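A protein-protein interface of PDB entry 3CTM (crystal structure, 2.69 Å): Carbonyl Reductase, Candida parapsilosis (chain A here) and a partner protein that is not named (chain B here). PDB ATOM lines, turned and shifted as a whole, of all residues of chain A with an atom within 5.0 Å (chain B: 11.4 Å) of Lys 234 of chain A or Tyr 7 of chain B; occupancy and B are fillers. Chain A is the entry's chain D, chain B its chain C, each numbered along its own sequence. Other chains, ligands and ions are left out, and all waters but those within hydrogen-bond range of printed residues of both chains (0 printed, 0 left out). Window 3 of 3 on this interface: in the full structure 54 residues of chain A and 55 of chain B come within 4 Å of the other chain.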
ATOM      1  N   ASP A 230     -13.183  -6.248  16.499  1.00  0.00           N
ATOM      2  CA  ASP A 230     -12.553  -5.941  17.782  1.00  0.00           C
ATOM      3  C   ASP A 230     -11.165  -6.568  17.869  1.00  0.00           C
ATOM      4  O   ASP A 230     -10.272  -6.031  18.541  1.00  0.00           O
ATOM      5  CB  ASP A 230     -13.442  -6.430  18.936  1.00  0.00           C
ATOM      6  CG  ASP A 230     -14.418  -5.357  19.443  1.00  0.00           C
ATOM      7  OD1 ASP A 230     -13.965  -4.345  20.025  1.00  0.00           O
ATOM      8  OD2 ASP A 230     -15.646  -5.538  19.281  1.00  0.00           O
ATOM      9  N   MET A 231     -10.969  -7.705  17.196  1.00  0.00           N
ATOM     10  CA  MET A 231      -9.647  -8.314  17.130  1.00  0.00           C
ATOM     11  C   MET A 231      -8.722  -7.488  16.240  1.00  0.00           C
ATOM     12  O   MET A 231      -7.727  -6.929  16.715  1.00  0.00           O
ATOM     13  CB  MET A 231      -9.779  -9.764  16.644  1.00  0.00           C
ATOM     14  CG  MET A 231      -8.548 -10.648  16.837  1.00  0.00           C
ATOM     15  SD  MET A 231      -7.493 -10.258  18.260  1.00  0.00           S
ATOM     16  CE  MET A 231      -6.182 -11.470  18.024  1.00  0.00           C
ATOM     17  N   LYS A 232      -9.068  -7.366  14.948  1.00  0.00           N
ATOM     18  CA  LYS A 232      -8.255  -6.607  13.999  1.00  0.00           C
ATOM     19  C   LYS A 232      -7.892  -5.227  14.538  1.00  0.00           C
ATOM     20  O   LYS A 232      -6.779  -4.736  14.310  1.00  0.00           O
ATOM     21  CB  LYS A 232      -8.995  -6.463  12.665  1.00  0.00           C
ATOM     22  CG  LYS A 232      -8.877  -7.648  11.721  1.00  0.00           C
ATOM     23  CD  LYS A 232      -9.433  -7.339  10.330  1.00  0.00           C
ATOM     24  CE  LYS A 232      -9.863  -8.615   9.616  1.00  0.00           C
ATOM     25  NZ  LYS A 232      -9.038  -8.894   8.393  1.00  0.00           N
ATOM     26  N   ALA A 233      -8.821  -4.584  15.256  1.00  0.00           N
ATOM     27  CA  ALA A 233      -8.536  -3.265  15.815  1.00  0.00           C
ATOM     28  C   ALA A 233      -7.344  -3.298  16.764  1.00  0.00           C
ATOM     29  O   ALA A 233      -6.598  -2.318  16.852  1.00  0.00           O
ATOM     30  CB  ALA A 233      -9.769  -2.711  16.533  1.00  0.00           C
ATOM     31  N   LYS A 234      -7.143  -4.413  17.473  1.00  0.00           N
ATOM     32  CA  LYS A 234      -6.026  -4.497  18.404  1.00  0.00           C
ATOM     33  C   LYS A 234      -4.694  -4.607  17.675  1.00  0.00           C
ATOM     34  O   LYS A 234      -3.661  -4.191  18.211  1.00  0.00           O
ATOM     35  CB  LYS A 234      -6.215  -5.678  19.351  1.00  0.00           C
ATOM     36  CG  LYS A 234      -6.843  -5.295  20.679  1.00  0.00           C
ATOM     37  CD  LYS A 234      -5.975  -4.266  21.401  1.00  0.00           C
ATOM     38  CE  LYS A 234      -6.807  -3.125  21.990  1.00  0.00           C
ATOM     39  NZ  LYS A 234      -5.991  -2.231  22.873  1.00  0.00           N
ATOM     40  N   TRP A 235      -4.690  -5.161  16.461  1.00  0.00           N
ATOM     41  CA  TRP A 235      -3.462  -5.138  15.671  1.00  0.00           C
ATOM     42  C   TRP A 235      -3.107  -3.710  15.272  1.00  0.00           C
ATOM     43  O   TRP A 235      -1.994  -3.244  15.534  1.00  0.00           O
ATOM     44  CB  TRP A 235      -3.604  -6.022  14.431  1.00  0.00           C
ATOM     45  CG  TRP A 235      -4.054  -7.397  14.734  1.00  0.00           C
ATOM     46  CD1 TRP A 235      -3.911  -8.058  15.909  1.00  0.00           C
ATOM     47  CD2 TRP A 235      -4.739  -8.294  13.847  1.00  0.00           C
ATOM     48  NE1 TRP A 235      -4.464  -9.315  15.817  1.00  0.00           N
ATOM     49  CE2 TRP A 235      -4.979  -9.482  14.559  1.00  0.00           C
ATOM     50  CE3 TRP A 235      -5.166  -8.208  12.521  1.00  0.00           C
ATOM     51  CZ2 TRP A 235      -5.628 -10.574  13.992  1.00  0.00           C
ATOM     52  CZ3 TRP A 235      -5.803  -9.293  11.959  1.00  0.00           C
ATOM     53  CH2 TRP A 235      -6.031 -10.460  12.694  1.00  0.00           C
ATOM     54  N   TRP A 236      -4.069  -2.991  14.679  1.00  0.00           N
ATOM     55  CA  TRP A 236      -3.838  -1.653  14.145  1.00  0.00           C
ATOM     56  C   TRP A 236      -3.180  -0.710  15.135  1.00  0.00           C
ATOM     57  O   TRP A 236      -2.441   0.190  14.728  1.00  0.00           O
ATOM     58  CB  TRP A 236      -5.149  -1.020  13.698  1.00  0.00           C
ATOM     59  CG  TRP A 236      -5.957  -1.834  12.765  1.00  0.00           C
ATOM     60  CD1 TRP A 236      -5.517  -2.800  11.927  1.00  0.00           C
ATOM     61  CD2 TRP A 236      -7.369  -1.737  12.568  1.00  0.00           C
ATOM     62  NE1 TRP A 236      -6.564  -3.319  11.211  1.00  0.00           N
ATOM     63  CE2 TRP A 236      -7.716  -2.685  11.587  1.00  0.00           C
ATOM     64  CE3 TRP A 236      -8.378  -0.936  13.130  1.00  0.00           C
ATOM     65  CZ2 TRP A 236      -9.031  -2.859  11.142  1.00  0.00           C
ATOM     66  CZ3 TRP A 236      -9.690  -1.114  12.694  1.00  0.00           C
ATOM     67  CH2 TRP A 236     -10.001  -2.069  11.710  1.00  0.00           C
ATOM     68  N   GLN A 237      -3.476  -0.840  16.422  1.00  0.00           N
ATOM     69  CA  GLN A 237      -2.876   0.091  17.368  1.00  0.00           C
ATOM     70  C   GLN A 237      -1.511  -0.354  17.830  1.00  0.00           C
ATOM     71  O   GLN A 237      -0.780   0.445  18.423  1.00  0.00           O
ATOM     72  CB  GLN A 237      -3.770   0.307  18.588  1.00  0.00           C
ATOM     73  CG  GLN A 237      -4.979  -0.583  18.663  1.00  0.00           C
ATOM     74  CD  GLN A 237      -6.056   0.011  19.556  1.00  0.00           C
ATOM     75  OE1 GLN A 237      -6.822  -0.714  20.183  1.00  0.00           O
ATOM     76  NE2 GLN A 237      -6.106   1.345  19.630  1.00  0.00           N
ATOM     77  N   LEU A 238      -1.154  -1.598  17.568  1.00  0.00           N
ATOM     78  CA  LEU A 238       0.152  -2.090  17.949  1.00  0.00           C
ATOM     79  C   LEU A 238       1.167  -1.984  16.824  1.00  0.00           C
ATOM     80  O   LEU A 238       2.368  -1.858  17.093  1.00  0.00           O
ATOM     81  CB  LEU A 238       0.026  -3.535  18.427  1.00  0.00           C
ATOM     82  CG  LEU A 238      -0.376  -3.616  19.903  1.00  0.00           C
ATOM     83  CD1 LEU A 238      -0.197  -5.038  20.412  1.00  0.00           C
ATOM     84  CD2 LEU A 238       0.425  -2.589  20.753  1.00  0.00           C
ATOM     85  N   GLU B   3     -13.633   6.179  18.427  1.00  0.00           N
ATOM     86  CA  GLU B   3     -12.580   6.097  17.420  1.00  0.00           C
ATOM     87  C   GLU B   3     -11.309   5.445  17.980  1.00  0.00           C
ATOM     88  O   GLU B   3     -10.962   5.650  19.144  1.00  0.00           O
ATOM     89  CB  GLU B   3     -12.258   7.482  16.861  1.00  0.00           C
ATOM     90  CG  GLU B   3     -12.853   7.734  15.482  1.00  0.00           C
ATOM     91  CD  GLU B   3     -13.001   6.453  14.647  1.00  0.00           C
ATOM     92  OE1 GLU B   3     -11.963   5.879  14.227  1.00  0.00           O
ATOM     93  OE2 GLU B   3     -14.158   6.029  14.401  1.00  0.00           O
ATOM     94  N   ILE B   4     -10.616   4.677  17.135  1.00  0.00           N
ATOM     95  CA  ILE B   4      -9.533   3.793  17.562  1.00  0.00           C
ATOM     96  C   ILE B   4      -8.195   4.516  17.446  1.00  0.00           C
ATOM     97  O   ILE B   4      -7.809   4.946  16.354  1.00  0.00           O
ATOM     98  CB  ILE B   4      -9.527   2.508  16.726  1.00  0.00           C
ATOM     99  CG1 ILE B   4     -10.695   1.612  17.122  1.00  0.00           C
ATOM    100  CG2 ILE B   4      -8.211   1.763  16.912  1.00  0.00           C
ATOM    101  CD1 ILE B   4     -10.459   0.831  18.411  1.00  0.00           C
ATOM    102  N   GLU B   5      -7.466   4.610  18.560  1.00  0.00           N
ATOM    103  CA  GLU B   5      -6.240   5.400  18.638  1.00  0.00           C
ATOM    104  C   GLU B   5      -5.012   4.513  18.835  1.00  0.00           C
ATOM    105  O   GLU B   5      -5.047   3.536  19.594  1.00  0.00           O
ATOM    106  CB  GLU B   5      -6.312   6.423  19.778  1.00  0.00           C
ATOM    107  CG  GLU B   5      -6.924   7.762  19.389  1.00  0.00           C
ATOM    108  CD  GLU B   5      -6.750   8.820  20.473  1.00  0.00           C
ATOM    109  OE1 GLU B   5      -6.750  10.028  20.140  1.00  0.00           O
ATOM    110  OE2 GLU B   5      -6.602   8.440  21.658  1.00  0.00           O
ATOM    111  N   SER B   6      -3.921   4.887  18.164  1.00  0.00           N
ATOM    112  CA  SER B   6      -2.689   4.114  18.174  1.00  0.00           C
ATOM    113  C   SER B   6      -2.068   4.062  19.566  1.00  0.00           C
ATOM    114  O   SER B   6      -2.154   5.011  20.346  1.00  0.00           O
ATOM    115  CB  SER B   6      -1.688   4.712  17.179  1.00  0.00           C
ATOM    116  OG  SER B   6      -0.338   4.480  17.565  1.00  0.00           O
ATOM    117  N   TYR B   7      -1.437   2.920  19.869  1.00  0.00           N
ATOM    118  CA  TYR B   7      -0.577   2.747  21.034  1.00  0.00           C
ATOM    119  C   TYR B   7       0.853   3.187  20.768  1.00  0.00           C
ATOM    120  O   TYR B   7       1.668   3.183  21.697  1.00  0.00           O
ATOM    121  CB  TYR B   7      -0.533   1.274  21.462  1.00  0.00           C
ATOM    122  CG  TYR B   7      -1.415   0.867  22.629  1.00  0.00           C
ATOM    123  CD1 TYR B   7      -2.777   1.188  22.657  1.00  0.00           C
ATOM    124  CD2 TYR B   7      -0.893   0.108  23.682  1.00  0.00           C
ATOM    125  CE1 TYR B   7      -3.589   0.793  23.722  1.00  0.00           C
ATOM    126  CE2 TYR B   7      -1.692  -0.294  24.745  1.00  0.00           C
ATOM    127  CZ  TYR B   7      -3.039   0.052  24.760  1.00  0.00           C
ATOM    128  OH  TYR B   7      -3.827  -0.348  25.814  1.00  0.00           O
ATOM    129  N   CYS B   8       1.180   3.528  19.519  1.00  0.00           N
ATOM    130  CA  CYS B   8       2.548   3.811  19.113  1.00  0.00           C
ATOM    131  C   CYS B   8       2.796   5.281  18.844  1.00  0.00           C
ATOM    132  O   CYS B   8       3.903   5.770  19.081  1.00  0.00           O
ATOM    133  CB  CYS B   8       2.910   3.003  17.854  1.00  0.00           C
ATOM    134  SG  CYS B   8       3.186   1.202  18.112  1.00  0.00           S
ATOM    135  N   ASN B   9       1.784   5.996  18.385  1.00  0.00           N
ATOM    136  CA  ASN B   9       1.957   7.353  17.899  1.00  0.00           C
ATOM    137  C   ASN B   9       0.578   7.904  17.604  1.00  0.00           C
ATOM    138  O   ASN B   9      -0.043   7.528  16.603  1.00  0.00           O
ATOM    139  CB  ASN B   9       2.839   7.390  16.644  1.00  0.00           C
ATOM    140  CG  ASN B   9       3.215   8.803  16.232  1.00  0.00           C
ATOM    141  OD1 ASN B   9       2.537   9.758  16.594  1.00  0.00           O
ATOM    142  ND2 ASN B   9       4.294   8.941  15.469  1.00  0.00           N
ATOM    143  N   LYS B  10       0.086   8.783  18.477  1.00  0.00           N
ATOM    144  CA  LYS B  10      -1.271   9.281  18.315  1.00  0.00           C
ATOM    145  C   LYS B  10      -1.406  10.214  17.123  1.00  0.00           C
ATOM    146  O   LYS B  10      -2.531  10.569  16.765  1.00  0.00           O
ATOM    147  CB  LYS B  10      -1.730   9.954  19.612  1.00  0.00           C
ATOM    148  CG  LYS B  10      -1.985   8.941  20.731  1.00  0.00           C
ATOM    149  CD  LYS B  10      -2.959   9.456  21.782  1.00  0.00           C
ATOM    150  CE  LYS B  10      -2.584   8.979  23.199  1.00  0.00           C
ATOM    151  NZ  LYS B  10      -2.463   7.486  23.321  1.00  0.00           N
ATOM    152  N   GLU B  11      -0.301  10.571  16.470  1.00  0.00           N
ATOM    153  CA  GLU B  11      -0.324  11.409  15.279  1.00  0.00           C
ATOM    154  C   GLU B  11      -0.668  10.641  14.015  1.00  0.00           C
ATOM    155  O   GLU B  11      -0.792  11.257  12.953  1.00  0.00           O
ATOM    156  CB  GLU B  11       1.021  12.101  15.118  1.00  0.00           C
ATOM    157  CG  GLU B  11       1.294  13.095  16.236  1.00  0.00           C
ATOM    158  CD  GLU B  11       0.553  14.402  16.004  1.00  0.00           C
ATOM    159  OE1 GLU B  11       0.735  14.985  14.911  1.00  0.00           O
ATOM    160  OE2 GLU B  11      -0.222  14.832  16.891  1.00  0.00           O
ATOM    161  N   LEU B  12      -0.809   9.316  14.107  1.00  0.00           N
ATOM    162  CA  LEU B  12      -1.333   8.520  13.005  1.00  0.00           C
ATOM    163  C   LEU B  12      -2.816   8.773  12.762  1.00  0.00           C
ATOM    164  O   LEU B  12      -3.328   8.390  11.704  1.00  0.00           O
ATOM    165  CB  LEU B  12      -1.130   7.035  13.292  1.00  0.00           C
ATOM    166  CG  LEU B  12       0.287   6.473  13.205  1.00  0.00           C
ATOM    167  CD1 LEU B  12       0.321   5.098  13.881  1.00  0.00           C
ATOM    168  CD2 LEU B  12       0.781   6.406  11.764  1.00  0.00           C
ATOM    169  N   GLY B  13      -3.514   9.383  13.724  1.00  0.00           N
ATOM    170  CA  GLY B  13      -4.932   9.630  13.615  1.00  0.00           C
ATOM    171  C   GLY B  13      -5.758   8.387  13.875  1.00  0.00           C
ATOM    172  O   GLY B  13      -5.232   7.320  14.204  1.00  0.00           O
ATOM    173  N   PRO B  14      -7.074   8.505  13.724  1.00  0.00           N
ATOM    174  CA  PRO B  14      -7.949   7.343  13.915  1.00  0.00           C
ATOM    175  C   PRO B  14      -7.499   6.156  13.078  1.00  0.00           C
ATOM    176  O   PRO B  14      -7.077   6.303  11.928  1.00  0.00           O
ATOM    177  CB  PRO B  14      -9.319   7.854  13.460  1.00  0.00           C
ATOM    178  CG  PRO B  14      -9.018   9.073  12.628  1.00  0.00           C
ATOM    179  CD  PRO B  14      -7.822   9.684  13.273  1.00  0.00           C
ATOM    180  N   LEU B  15      -7.614   5.005  13.645  1.00  0.00           N
ATOM    181  CA  LEU B  15      -7.079   3.860  12.939  1.00  0.00           C
ATOM    182  C   LEU B  15      -8.180   3.059  12.247  1.00  0.00           C
ATOM    183  O   LEU B  15      -9.359   3.165  12.587  1.00  0.00           O
ATOM    184  CB  LEU B  15      -6.307   2.967  13.912  1.00  0.00           C
ATOM    185  CG  LEU B  15      -5.060   3.606  14.524  1.00  0.00           C
ATOM    186  CD1 LEU B  15      -4.337   2.615  15.385  1.00  0.00           C
ATOM    187  CD2 LEU B  15      -4.124   4.154  13.444  1.00  0.00           C
ATOM    188  N   PRO B  16      -7.844   2.268  11.227  1.00  0.00           N
ATOM    189  CA  PRO B  16      -6.512   2.115  10.629  1.00  0.00           C
ATOM    190  C   PRO B  16      -6.134   3.255   9.684  1.00  0.00           C
ATOM    191  O   PRO B  16      -7.018   3.759   8.982  1.00  0.00           O
ATOM    192  CB  PRO B  16      -6.640   0.805   9.852  1.00  0.00           C
ATOM    193  CG  PRO B  16      -8.096   0.740   9.467  1.00  0.00           C
ATOM    194  CD  PRO B  16      -8.863   1.452  10.545  1.00  0.00           C
ATOM    195  N   THR B  17      -4.851   3.645   9.665  1.00  0.00           N
ATOM    196  CA  THR B  17      -4.297   4.335   8.504  1.00  0.00           C
ATOM    197  C   THR B  17      -4.628   3.492   7.284  1.00  0.00           C
ATOM    198  O   THR B  17      -4.891   2.292   7.404  1.00  0.00           O
ATOM    199  CB  THR B  17      -2.790   4.513   8.617  1.00  0.00           C
ATOM    200  OG1 THR B  17      -2.178   3.216   8.691  1.00  0.00           O
ATOM    201  CG2 THR B  17      -2.417   5.355   9.840  1.00  0.00           C
ATOM    202  N   ALA B 202      11.453   4.893  12.922  1.00  0.00           N
ATOM    203  CA  ALA B 202      10.367   4.137  12.312  1.00  0.00           C
ATOM    204  C   ALA B 202       9.041   4.454  12.990  1.00  0.00           C
ATOM    205  O   ALA B 202       8.038   4.709  12.321  1.00  0.00           O
ATOM    206  CB  ALA B 202      10.668   2.640  12.388  1.00  0.00           C
ATOM    207  N   ILE B 203       9.040   4.467  14.325  1.00  0.00           N
ATOM    208  CA  ILE B 203       7.852   4.804  15.101  1.00  0.00           C
ATOM    209  C   ILE B 203       7.547   6.303  15.023  1.00  0.00           C
ATOM    210  O   ILE B 203       6.403   6.698  14.766  1.00  0.00           O
ATOM    211  CB  ILE B 203       8.039   4.344  16.552  1.00  0.00           C
ATOM    212  CG1 ILE B 203       8.117   2.823  16.595  1.00  0.00           C
ATOM    213  CG2 ILE B 203       6.917   4.880  17.435  1.00  0.00           C
ATOM    214  CD1 ILE B 203       8.851   2.299  17.821  1.00  0.00           C
ATOM    215  N   GLU B 204       8.555   7.156  15.261  1.00  0.00           N
ATOM    216  CA  GLU B 204       8.329   8.598  15.205  1.00  0.00           C
ATOM    217  C   GLU B 204       7.768   9.030  13.859  1.00  0.00           C
ATOM    218  O   GLU B 204       6.873   9.879  13.801  1.00  0.00           O
ATOM    219  CB  GLU B 204       9.625   9.360  15.510  1.00  0.00           C
ATOM    220  CG  GLU B 204       9.438  10.755  16.179  1.00  0.00           C
ATOM    221  CD  GLU B 204      10.552  11.789  15.831  1.00  0.00           C
ATOM    222  OE1 GLU B 204      11.613  11.807  16.510  1.00  0.00           O
ATOM    223  OE2 GLU B 204      10.368  12.596  14.881  1.00  0.00           O
ATOM    224  N   ALA B 206       6.225   7.241  11.531  1.00  0.00           N
ATOM    225  CA  ALA B 206       5.209   6.340  10.987  1.00  0.00           C
ATOM    226  C   ALA B 206       4.078   7.040  10.241  1.00  0.00           C
ATOM    227  O   ALA B 206       3.626   6.498   9.217  1.00  0.00           O
ATOM    228  CB  ALA B 206       4.639   5.470  12.115  1.00  0.00           C
ATOM    229  N   PRO B 207       3.575   8.200  10.669  1.00  0.00           N
ATOM    230  CA  PRO B 207       2.560   8.875   9.849  1.00  0.00           C
ATOM    231  C   PRO B 207       3.053   9.256   8.463  1.00  0.00           C
ATOM    232  O   PRO B 207       2.220   9.389   7.559  1.00  0.00           O
ATOM    233  CB  PRO B 207       2.195  10.115  10.678  1.00  0.00           C
ATOM    234  CG  PRO B 207       2.515   9.738  12.075  1.00  0.00           C
ATOM    235  CD  PRO B 207       3.714   8.837  11.997  1.00  0.00           C
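No residue of chain B comes within 4 Å of Met 231 of chain A. No residue of chain B comes within 4 Å of Ala 233 of chain A. Of the printed residues of chain B, Lys 234 of chain A touches Tyr 7. Of chain B, only Leu 15 and Pro 16 come within 4 Å of Trp 236 of chain A. Printed residues of chain A within 4 Å of Ile 4 of chain B: Gln 237 (3.5 Å). Of the printed residues of chain A, Ser 6 of chain B touches Gln 237. Tyr 7 of chain B touches just these residues of chain A: Lys 234 (3.95 Å) and Gln 237 (2.9 Å). Of the printed residues of chain A, Cys 8 of chain B touches Gln 237 and Leu 238. Pro 14 of chain B touches none of the printed residues of chain A. Of the printed residues of chain A, Pro 16 of chain B touches Trp 236 (3.4 Å). Pro 207 of chain B touches none of the printed residues of chain A.
The backbone NH of Tyr 7 of chain B sits at hydrogen-bond distance from the backbone carbonyl oxygen of Gln 237 of chain A (2.9 Å). NE2 of Gln 237 of chain A sits at hydrogen-bond distance from O of Glu 5 of chain B, at 2.4 Å. The side-chain sulfur of Cys 8 of chain B is in hydrogen-bond range of the backbone carbonyl oxygen of Leu 238 of chain A (3.3 Å).
Of the 9 printed residues of chain A, 4 touch a printed residue of chain B. Hydrophobic or aromatic side chains of chain A within 4 Å of the printed part of chain B: Trp 236. Of the 20 printed residues of chain B, 7 touch a printed residue of chain A. Hydrophobic or aromatic side chains of chain B that line the printed part of chain A: Ile 4, Tyr 7, Leu 15 and Pro 16. Along chain B the printed residues that touch a printed residue of chain A span positions 4 to 16. Among the printed residues, no Asp or Glu carboxylate lies within 4 Å of a Lys or Arg side-chain nitrogen of the other chain.
O of Ile 4 of chain B is in hydrogen-bond range of N of Leu 15 of chain B (2.7 Å). The backbone carbonyl oxygen (O) of Lys 232 of chain A lies close to the indole nitrogen (NE1) of Trp 236 of chain A. The side-chain amide oxygen (OE1) of Gln 237 of chain A sits close to the side-chain amino group (NZ) of Lys 234 of chain A. The backbone NH of Cys 8 of chain B is in hydrogen-bond range of the side-chain hydroxyl of Ser 6 of chain B, 2.7 Å away. The backbone NH of Asn 9 of chain B is in hydrogen-bond range of the side-chain hydroxyl of Ser 6 of chain B (2.7 Å).
Among the printed residues, pairs that only touch across the chains: Trp 236 of chain A with Leu 15 of chain B (3.1 Å), Trp 236 of chain A with Pro 16 of chain B (3.4 Å), Gln 237 of chain A with Ile 4 of chain B (3.5 Å), Gln 237 of chain A with Leu 15 of chain B (3.5 Å), Gln 237 of chain A with Cys 8 of chain B (3.8 Å), Lys 234 of chain A with Tyr 7 of chain B (3.95 Å) and Gln 237 of chain A with Ser 6 of chain B (3.98 Å).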
